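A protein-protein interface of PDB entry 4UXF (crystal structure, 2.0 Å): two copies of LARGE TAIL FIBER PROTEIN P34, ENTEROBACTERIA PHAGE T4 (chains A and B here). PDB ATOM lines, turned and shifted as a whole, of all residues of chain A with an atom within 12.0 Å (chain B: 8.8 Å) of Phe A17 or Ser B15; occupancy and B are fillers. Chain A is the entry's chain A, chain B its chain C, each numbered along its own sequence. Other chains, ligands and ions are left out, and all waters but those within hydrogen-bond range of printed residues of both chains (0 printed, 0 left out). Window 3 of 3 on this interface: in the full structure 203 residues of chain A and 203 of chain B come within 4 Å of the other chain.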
ATOM      1  N   PRO A  14      11.269   8.178  -9.449  1.00  0.00           N
ATOM      2  CA  PRO A  14      12.012   8.983  -8.460  1.00  0.00           C
ATOM      3  C   PRO A  14      13.515   8.624  -8.382  1.00  0.00           C
ATOM      4  O   PRO A  14      14.333   9.339  -8.967  1.00  0.00           O
ATOM      5  CB  PRO A  14      11.255   8.714  -7.145  1.00  0.00           C
ATOM      6  CG  PRO A  14      10.504   7.426  -7.362  1.00  0.00           C
ATOM      7  CD  PRO A  14      10.514   7.075  -8.829  1.00  0.00           C
ATOM      8  N   SER A  15      13.856   7.520  -7.699  1.00  0.00           N
ATOM      9  CA  SER A  15      15.220   6.969  -7.651  1.00  0.00           C
ATOM     10  C   SER A  15      15.436   5.906  -8.741  1.00  0.00           C
ATOM     11  O   SER A  15      16.356   5.094  -8.659  1.00  0.00           O
ATOM     12  CB  SER A  15      15.495   6.370  -6.265  1.00  0.00           C
ATOM     13  OG  SER A  15      14.653   5.260  -6.003  1.00  0.00           O
ATOM     14  N   GLN A  16      14.566   5.918  -9.752  1.00  0.00           N
ATOM     15  CA  GLN A  16      14.778   5.203 -11.003  1.00  0.00           C
ATOM     16  C   GLN A  16      15.777   5.946 -11.895  1.00  0.00           C
ATOM     17  O   GLN A  16      16.136   5.435 -12.949  1.00  0.00           O
ATOM     18  CB  GLN A  16      13.454   5.052 -11.780  1.00  0.00           C
ATOM     19  CG  GLN A  16      12.306   4.371 -11.041  1.00  0.00           C
ATOM     20  CD  GLN A  16      12.415   2.857 -11.022  1.00  0.00           C
ATOM     21  OE1 GLN A  16      13.500   2.300 -10.855  1.00  0.00           O
ATOM     22  NE2 GLN A  16      11.281   2.185 -11.178  1.00  0.00           N
ATOM     23  N   PHE A  17      16.174   7.163 -11.511  1.00  0.00           N
ATOM     24  CA  PHE A  17      17.254   7.898 -12.177  1.00  0.00           C
ATOM     25  C   PHE A  17      18.456   8.084 -11.233  1.00  0.00           C
ATOM     26  O   PHE A  17      18.333   7.878 -10.006  1.00  0.00           O
ATOM     27  CB  PHE A  17      16.733   9.244 -12.697  1.00  0.00           C
ATOM     28  CG  PHE A  17      15.567   9.110 -13.636  1.00  0.00           C
ATOM     29  CD1 PHE A  17      15.748   8.604 -14.921  1.00  0.00           C
ATOM     30  CD2 PHE A  17      14.285   9.465 -13.234  1.00  0.00           C
ATOM     31  CE1 PHE A  17      14.681   8.470 -15.795  1.00  0.00           C
ATOM     32  CE2 PHE A  17      13.213   9.332 -14.106  1.00  0.00           C
ATOM     33  CZ  PHE A  17      13.411   8.830 -15.385  1.00  0.00           C
ATOM     34  N   ILE A  18      19.614   8.441 -11.806  1.00  0.00           N
ATOM     35  CA  ILE A  18      20.848   8.566 -11.015  1.00  0.00           C
ATOM     36  C   ILE A  18      21.065  10.002 -10.546  1.00  0.00           C
ATOM     37  O   ILE A  18      21.086  10.948 -11.348  1.00  0.00           O
ATOM     38  CB  ILE A  18      22.123   8.066 -11.749  1.00  0.00           C
ATOM     39  CG1 ILE A  18      21.954   6.604 -12.185  1.00  0.00           C
ATOM     40  CG2 ILE A  18      23.354   8.207 -10.835  1.00  0.00           C
ATOM     41  CD1 ILE A  18      23.042   6.095 -13.104  1.00  0.00           C
ATOM     42  N   ARG A  19      21.263  10.120  -9.237  1.00  0.00           N
ATOM     43  CA  ARG A  19      21.503  11.392  -8.578  1.00  0.00           C
ATOM     44  C   ARG A  19      22.894  11.928  -8.951  1.00  0.00           C
ATOM     45  O   ARG A  19      23.862  11.168  -9.072  1.00  0.00           O
ATOM     46  CB  ARG A  19      21.384  11.219  -7.058  1.00  0.00           C
ATOM     47  CG  ARG A  19      21.140  12.488  -6.281  1.00  0.00           C
ATOM     48  CD  ARG A  19      19.672  12.892  -6.190  1.00  0.00           C
ATOM     49  NE  ARG A  19      19.593  14.101  -5.374  1.00  0.00           N
ATOM     50  CZ  ARG A  19      19.694  14.146  -4.043  1.00  0.00           C
ATOM     51  NH1 ARG A  19      19.837  13.045  -3.316  1.00  0.00           N
ATOM     52  NH2 ARG A  19      19.631  15.315  -3.419  1.00  0.00           N
ATOM     53  N   ARG A  20      22.977  13.242  -9.109  1.00  0.00           N
ATOM     54  CA  ARG A  20      24.132  13.894  -9.707  1.00  0.00           C
ATOM     55  C   ARG A  20      25.000  14.634  -8.689  1.00  0.00           C
ATOM     56  O   ARG A  20      25.975  15.265  -9.077  1.00  0.00           O
ATOM     57  CB  ARG A  20      23.627  14.877 -10.759  1.00  0.00           C
ATOM     58  CG  ARG A  20      24.553  15.085 -11.931  1.00  0.00           C
ATOM     59  CD  ARG A  20      24.220  16.373 -12.653  1.00  0.00           C
ATOM     60  NE  ARG A  20      24.813  17.516 -11.970  1.00  0.00           N
ATOM     61  CZ  ARG A  20      24.934  18.741 -12.482  1.00  0.00           C
ATOM     62  NH1 ARG A  20      24.491  19.033 -13.706  1.00  0.00           N
ATOM     63  NH2 ARG A  20      25.505  19.690 -11.752  1.00  0.00           N
ATOM     64  N   ASP A  21      24.649  14.551  -7.404  1.00  0.00           N
ATOM     65  CA  ASP A  21      25.275  15.369  -6.342  1.00  0.00           C
ATOM     66  C   ASP A  21      25.676  14.606  -5.080  1.00  0.00           C
ATOM     67  O   ASP A  21      26.372  15.168  -4.224  1.00  0.00           O
ATOM     68  CB  ASP A  21      24.332  16.512  -5.930  1.00  0.00           C
ATOM     69  CG  ASP A  21      22.945  16.010  -5.507  1.00  0.00           C
ATOM     70  OD1 ASP A  21      22.119  15.742  -6.407  1.00  0.00           O
ATOM     71  OD2 ASP A  21      22.693  15.854  -4.291  1.00  0.00           O
ATOM     72  N   ILE A  22      25.224  13.361  -4.935  1.00  0.00           N
ATOM     73  CA  ILE A  22      25.692  12.491  -3.853  1.00  0.00           C
ATOM     74  C   ILE A  22      26.028  11.078  -4.365  1.00  0.00           C
ATOM     75  O   ILE A  22      25.768  10.734  -5.537  1.00  0.00           O
ATOM     76  CB  ILE A  22      24.671  12.423  -2.690  1.00  0.00           C
ATOM     77  CG1 ILE A  22      23.284  12.002  -3.189  1.00  0.00           C
ATOM     78  CG2 ILE A  22      24.597  13.765  -1.976  1.00  0.00           C
ATOM     79  CD1 ILE A  22      22.409  11.446  -2.088  1.00  0.00           C
ATOM     80  N   ALA A  23      26.636  10.294  -3.472  1.00  0.00           N
ATOM     81  CA  ALA A  23      26.984   8.894  -3.727  1.00  0.00           C
ATOM     82  C   ALA A  23      25.799   8.113  -4.291  1.00  0.00           C
ATOM     83  O   ALA A  23      24.693   8.195  -3.745  1.00  0.00           O
ATOM     84  CB  ALA A  23      27.473   8.235  -2.439  1.00  0.00           C
ATOM     85  N   GLN A  24      26.039   7.374  -5.373  1.00  0.00           N
ATOM     86  CA  GLN A  24      25.010   6.580  -6.045  1.00  0.00           C
ATOM     87  C   GLN A  24      25.527   5.217  -6.472  1.00  0.00           C
ATOM     88  O   GLN A  24      26.348   5.134  -7.387  1.00  0.00           O
ATOM     89  CB  GLN A  24      24.532   7.304  -7.301  1.00  0.00           C
ATOM     90  CG  GLN A  24      23.772   8.577  -7.029  1.00  0.00           C
ATOM     91  CD  GLN A  24      22.449   8.323  -6.330  1.00  0.00           C
ATOM     92  OE1 GLN A  24      21.497   7.850  -6.944  1.00  0.00           O
ATOM     93  NE2 GLN A  24      22.381   8.660  -5.048  1.00  0.00           N
ATOM     94  N   THR A  25      25.050   4.153  -5.828  1.00  0.00           N
ATOM     95  CA  THR A  25      25.182   2.817  -6.394  1.00  0.00           C
ATOM     96  C   THR A  25      24.297   2.706  -7.629  1.00  0.00           C
ATOM     97  O   THR A  25      23.117   3.015  -7.573  1.00  0.00           O
ATOM     98  CB  THR A  25      24.776   1.720  -5.402  1.00  0.00           C
ATOM     99  OG1 THR A  25      25.635   1.765  -4.260  1.00  0.00           O
ATOM    100  CG2 THR A  25      24.860   0.339  -6.054  1.00  0.00           C
ATOM    101  N   VAL A  26      24.870   2.251  -8.733  1.00  0.00           N
ATOM    102  CA  VAL A  26      24.141   2.026  -9.978  1.00  0.00           C
ATOM    103  C   VAL A  26      24.033   0.521 -10.208  1.00  0.00           C
ATOM    104  O   VAL A  26      25.006  -0.197 -10.003  1.00  0.00           O
ATOM    105  CB  VAL A  26      24.881   2.681 -11.150  1.00  0.00           C
ATOM    106  CG1 VAL A  26      24.192   2.422 -12.487  1.00  0.00           C
ATOM    107  CG2 VAL A  26      25.039   4.166 -10.871  1.00  0.00           C
ATOM    108  N   ASN A  27      22.847   0.047 -10.602  1.00  0.00           N
ATOM    109  CA  ASN A  27      22.628  -1.381 -10.890  1.00  0.00           C
ATOM    110  C   ASN A  27      22.224  -1.673 -12.337  1.00  0.00           C
ATOM    111  O   ASN A  27      21.941  -2.824 -12.678  1.00  0.00           O
ATOM    112  CB  ASN A  27      21.640  -1.981  -9.894  1.00  0.00           C
ATOM    113  CG  ASN A  27      22.005  -1.676  -8.452  1.00  0.00           C
ATOM    114  OD1 ASN A  27      21.327  -0.906  -7.785  1.00  0.00           O
ATOM    115  ND2 ASN A  27      23.091  -2.259  -7.972  1.00  0.00           N
ATOM    116  N   GLY A  28      22.223  -0.643 -13.186  1.00  0.00           N
ATOM    117  CA  GLY A  28      22.197  -0.822 -14.641  1.00  0.00           C
ATOM    118  C   GLY A  28      23.609  -0.899 -15.230  1.00  0.00           C
ATOM    119  O   GLY A  28      24.578  -0.425 -14.610  1.00  0.00           O
ATOM    120  N   LEU A  30      25.899   0.711 -17.741  1.00  0.00           N
ATOM    121  CA  LEU A  30      26.109   1.930 -18.525  1.00  0.00           C
ATOM    122  C   LEU A  30      27.043   1.731 -19.716  1.00  0.00           C
ATOM    123  O   LEU A  30      28.101   1.123 -19.574  1.00  0.00           O
ATOM    124  CB  LEU A  30      26.703   3.024 -17.641  1.00  0.00           C
ATOM    125  CG  LEU A  30      25.904   3.438 -16.407  1.00  0.00           C
ATOM    126  CD1 LEU A  30      26.757   4.227 -15.419  1.00  0.00           C
ATOM    127  CD2 LEU A  30      24.679   4.247 -16.825  1.00  0.00           C
ATOM    128  N   PRO B  14      10.703  12.575 -23.709  1.00  0.00           N
ATOM    129  CA  PRO B  14      10.827  11.428 -22.820  1.00  0.00           C
ATOM    130  C   PRO B  14      11.715  11.771 -21.623  1.00  0.00           C
ATOM    131  O   PRO B  14      12.005  12.951 -21.403  1.00  0.00           O
ATOM    132  CB  PRO B  14      11.497  10.391 -23.725  1.00  0.00           C
ATOM    133  CG  PRO B  14      12.371  11.209 -24.629  1.00  0.00           C
ATOM    134  CD  PRO B  14      11.805  12.611 -24.685  1.00  0.00           C
ATOM    135  N   SER B  15      12.120  10.763 -20.848  1.00  0.00           N
ATOM    136  CA  SER B  15      13.198  10.935 -19.876  1.00  0.00           C
ATOM    137  C   SER B  15      14.526  10.837 -20.630  1.00  0.00           C
ATOM    138  O   SER B  15      14.787   9.858 -21.327  1.00  0.00           O
ATOM    139  CB  SER B  15      13.129   9.896 -18.752  1.00  0.00           C
ATOM    140  OG  SER B  15      13.730   8.671 -19.134  1.00  0.00           O
ATOM    141  N   GLN B  16      15.327  11.890 -20.527  1.00  0.00           N
ATOM    142  CA  GLN B  16      16.715  11.888 -20.960  1.00  0.00           C
ATOM    143  C   GLN B  16      17.504  12.002 -19.670  1.00  0.00           C
ATOM    144  O   GLN B  16      18.245  12.963 -19.453  1.00  0.00           O
ATOM    145  CB  GLN B  16      16.993  13.077 -21.873  1.00  0.00           C
ATOM    146  CG  GLN B  16      16.142  13.112 -23.137  1.00  0.00           C
ATOM    147  CD  GLN B  16      15.882  14.521 -23.650  1.00  0.00           C
ATOM    148  OE1 GLN B  16      16.207  15.518 -22.997  1.00  0.00           O
ATOM    149  NE2 GLN B  16      15.277  14.609 -24.828  1.00  0.00           N
ATOM    150  N   PHE B  17      17.287  11.025 -18.793  1.00  0.00           N
ATOM    151  CA  PHE B  17      17.974  10.930 -17.513  1.00  0.00           C
ATOM    152  C   PHE B  17      18.454   9.491 -17.379  1.00  0.00           C
ATOM    153  O   PHE B  17      17.754   8.565 -17.797  1.00  0.00           O
ATOM    154  CB  PHE B  17      17.039  11.298 -16.359  1.00  0.00           C
ATOM    155  CG  PHE B  17      16.852  12.777 -16.173  1.00  0.00           C
ATOM    156  CD1 PHE B  17      17.796  13.530 -15.477  1.00  0.00           C
ATOM    157  CD2 PHE B  17      15.722  13.424 -16.675  1.00  0.00           C
ATOM    158  CE1 PHE B  17      17.628  14.898 -15.298  1.00  0.00           C
ATOM    159  CE2 PHE B  17      15.547  14.791 -16.496  1.00  0.00           C
ATOM    160  CZ  PHE B  17      16.502  15.527 -15.808  1.00  0.00           C
ATOM    161  N   ILE B  18      19.648   9.303 -16.816  1.00  0.00           N
ATOM    162  CA  ILE B  18      20.241   7.970 -16.784  1.00  0.00           C
ATOM    163  C   ILE B  18      19.455   7.182 -15.769  1.00  0.00           C
ATOM    164  O   ILE B  18      19.399   7.557 -14.596  1.00  0.00           O
ATOM    165  CB  ILE B  18      21.746   7.907 -16.382  1.00  0.00           C
ATOM    166  CG1 ILE B  18      22.672   8.454 -17.470  1.00  0.00           C
ATOM    167  CG2 ILE B  18      22.178   6.454 -16.195  1.00  0.00           C
ATOM    168  CD1 ILE B  18      22.656   9.945 -17.626  1.00  0.00           C
ATOM    169  N   ARG B  19      18.870   6.089 -16.238  1.00  0.00           N
ATOM    170  CA  ARG B  19      18.245   5.123 -15.353  1.00  0.00           C
ATOM    171  C   ARG B  19      19.288   4.417 -14.499  1.00  0.00           C
ATOM    172  O   ARG B  19      20.255   3.823 -15.001  1.00  0.00           O
ATOM    173  CB  ARG B  19      17.427   4.085 -16.122  1.00  0.00           C
ATOM    174  CG  ARG B  19      16.267   4.647 -16.945  1.00  0.00           C
ATOM    175  CD  ARG B  19      15.081   5.074 -16.085  1.00  0.00           C
ATOM    176  NE  ARG B  19      14.515   3.958 -15.323  1.00  0.00           N
ATOM    177  CZ  ARG B  19      13.777   2.975 -15.840  1.00  0.00           C
ATOM    178  NH1 ARG B  19      13.493   2.921 -17.143  1.00  0.00           N
ATOM    179  NH2 ARG B  19      13.319   2.018 -15.046  1.00  0.00           N
ATOM    180  N   ARG B  20      19.043   4.479 -13.196  1.00  0.00           N
ATOM    181  CA  ARG B  20      19.855   3.853 -12.169  1.00  0.00           C
ATOM    182  C   ARG B  20      19.593   2.347 -12.030  1.00  0.00           C
ATOM    183  O   ARG B  20      20.232   1.682 -11.205  1.00  0.00           O
ATOM    184  CB  ARG B  20      19.553   4.564 -10.844  1.00  0.00           C
ATOM    185  CG  ARG B  20      20.448   4.229  -9.674  1.00  0.00           C
ATOM    186  CD  ARG B  20      20.186   5.154  -8.502  1.00  0.00           C
ATOM    187  NE  ARG B  20      20.594   4.508  -7.259  1.00  0.00           N
ATOM    188  CZ  ARG B  20      19.916   3.540  -6.634  1.00  0.00           C
ATOM    189  NH1 ARG B  20      18.753   3.085  -7.111  1.00  0.00           N
ATOM    190  NH2 ARG B  20      20.409   3.016  -5.511  1.00  0.00           N
ATOM    191  N   ASP B  21      18.676   1.795 -12.827  1.00  0.00           N
ATOM    192  CA  ASP B  21      18.167   0.436 -12.579  1.00  0.00           C
ATOM    193  C   ASP B  21      18.331  -0.568 -13.720  1.00  0.00           C
ATOM    194  O   ASP B  21      18.351  -1.770 -13.457  1.00  0.00           O
ATOM    195  CB  ASP B  21      16.695   0.488 -12.092  1.00  0.00           C
ATOM    196  CG  ASP B  21      15.749   1.200 -13.076  1.00  0.00           C
ATOM    197  OD1 ASP B  21      15.965   2.388 -13.399  1.00  0.00           O
ATOM    198  OD2 ASP B  21      14.763   0.570 -13.513  1.00  0.00           O
ATOM    199  N   ILE B  22      18.440  -0.100 -14.967  1.00  0.00           N
ATOM    200  CA  ILE B  22      18.603  -0.994 -16.133  1.00  0.00           C
ATOM    201  C   ILE B  22      19.648  -0.422 -17.114  1.00  0.00           C
ATOM    202  O   ILE B  22      20.196   0.658 -16.876  1.00  0.00           O
ATOM    203  CB  ILE B  22      17.241  -1.347 -16.834  1.00  0.00           C
ATOM    204  CG1 ILE B  22      16.728  -0.241 -17.784  1.00  0.00           C
ATOM    205  CG2 ILE B  22      16.162  -1.747 -15.825  1.00  0.00           C
ATOM    206  CD1 ILE B  22      16.590   1.136 -17.187  1.00  0.00           C
ATOM    207  N   GLN B  24      21.731   1.391 -19.832  1.00  0.00           N
ATOM    208  CA  GLN B  24      21.610   2.747 -20.341  1.00  0.00           C
ATOM    209  C   GLN B  24      22.790   3.123 -21.195  1.00  0.00           C
ATOM    210  O   GLN B  24      23.927   3.085 -20.728  1.00  0.00           O
ATOM    211  CB  GLN B  24      21.572   3.740 -19.180  1.00  0.00           C
ATOM    212  CG  GLN B  24      20.335   3.658 -18.312  1.00  0.00           C
ATOM    213  CD  GLN B  24      19.075   4.045 -19.067  1.00  0.00           C
ATOM    214  OE1 GLN B  24      18.835   5.223 -19.337  1.00  0.00           O
ATOM    215  NE2 GLN B  24      18.253   3.057 -19.382  1.00  0.00           N
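Of the 10 printed residues of chain B, 8 touch a printed residue of chain A. Hydrophobic or aromatic side chains of chain A that line the printed part of chain B: Phe A17, Ile A18 and Leu A30. Among the printed residues, 20 pairs touch across the chains.
The guanidinium group (NH1) of Arg B20 is in hydrogen-bond range of the backbone carbonyl oxygen (O) of Ser A15 (3.5 Å). The backbone NH (N) of Asn A27 is in hydrogen-bond range of the backbone carbonyl oxygen (O) of Arg B20, at 3.1 Å. The guanidinium group (NE) of Arg B20 lies close to the side-chain amide oxygen (OE1) of Gln A24, at 3.5 Å. O of Thr A25 is in hydrogen-bond range of NE of Arg B20, at 2.9 Å. O of Ile B18 lies within hydrogen-bond range of N of Ile A18, 2.9 Å away. OD2 of Asp B21 lies close to OE1 of Gln A16 (3.4 Å). The backbone carbonyl oxygen of Gln A16 is in hydrogen-bond range of the backbone NH of Arg B20 (3.1 Å). NE of Arg B19 sits close to O of Gln A16 (3.2 Å).
Among the printed residues, merely in contact across the chains: Phe A17 with Ile B18 (3.3 Å), Leu A30 with Gln B24 (3.3 Å), Phe A17 with Phe B17 (3.3 Å), Gly A28 with Ile B22 (3.3 Å), Leu A30 with Ile B18 (3.4 Å), Ile A18 with Arg B20 (3.4 Å), Phe A17 with Arg B19 (3.4 Å), Phe A17 with Ser B15 (3.5 Å), Phe A17 with Arg B20 (3.6 Å), Gly A28 with Arg B20 (3.6 Å), Asn A27 with Asp B21 (3.8 Å) and Gly A28 with Asp B21 (3.9 Å).
Of chain A, only Phe A17 (3.5 Å) comes within 4 Å of Ser B15. No residue of chain A comes within 4 Å of Pro B14. No residue of chain A comes within 4 Å of Gln B16. Phe B17 touches just one residue of chain A: Phe A17. Ile B18 touches three residues of chain A. Of the printed residues of chain A, Arg B19 touches Gln A16 (3.2 Å) and Phe A17 (3.4 Å). Of the printed residues of chain A, Arg B20 touches Ser A15, Gln A16, Phe A17, Ile A18, Gln A24, Thr A25, Asn A27 and Gly A28. Of the printed residues of chain B, Ser A15 touches Arg B20 (3.5 Å). Of the printed residues of chain A, Ile B22 touches Gly A28. Of the printed residues of chain B, Leu A30 touches Ile B18 (3.4 Å) and Gln B24 (3.3 Å). Of the printed residues of chain B, Gly A28 touches Arg B20, Asp B21 and Ile B22. Printed residues of chain B within 4 Å of Gln A24: Arg B20 (3.4 Å). Pro A14 touches none of the printed residues of chain B.
N of Arg A19 lies within hydrogen-bond range of OE1 of Gln A24 (3.2 Å). NH2 of Arg B19 lies within salt-bridge range of OD2 of Asp B21, 2.6 Å away. The backbone NH (N) of Arg B19 is in hydrogen-bond range of the side-chain amide oxygen (OE1) of Gln B24.
Ser A15 touches Arg B20, but with the chains exchanged Arg A20 does not touch Ser B15 (13.7 Å). Phe A17 touches Ile B18, but with the chains exchanged Ile A18 does not touch Phe B17 (5.8 Å). Phe A17 touches Arg B20, but with the chains exchanged Arg A20 does not touch Phe B17 (7.3 Å). Ile A18 touches its own counterpart, Ile B18. Of the 20 pairs that touch across the chains among the printed residues, 2 have their exchanged pair printed and touching as well.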
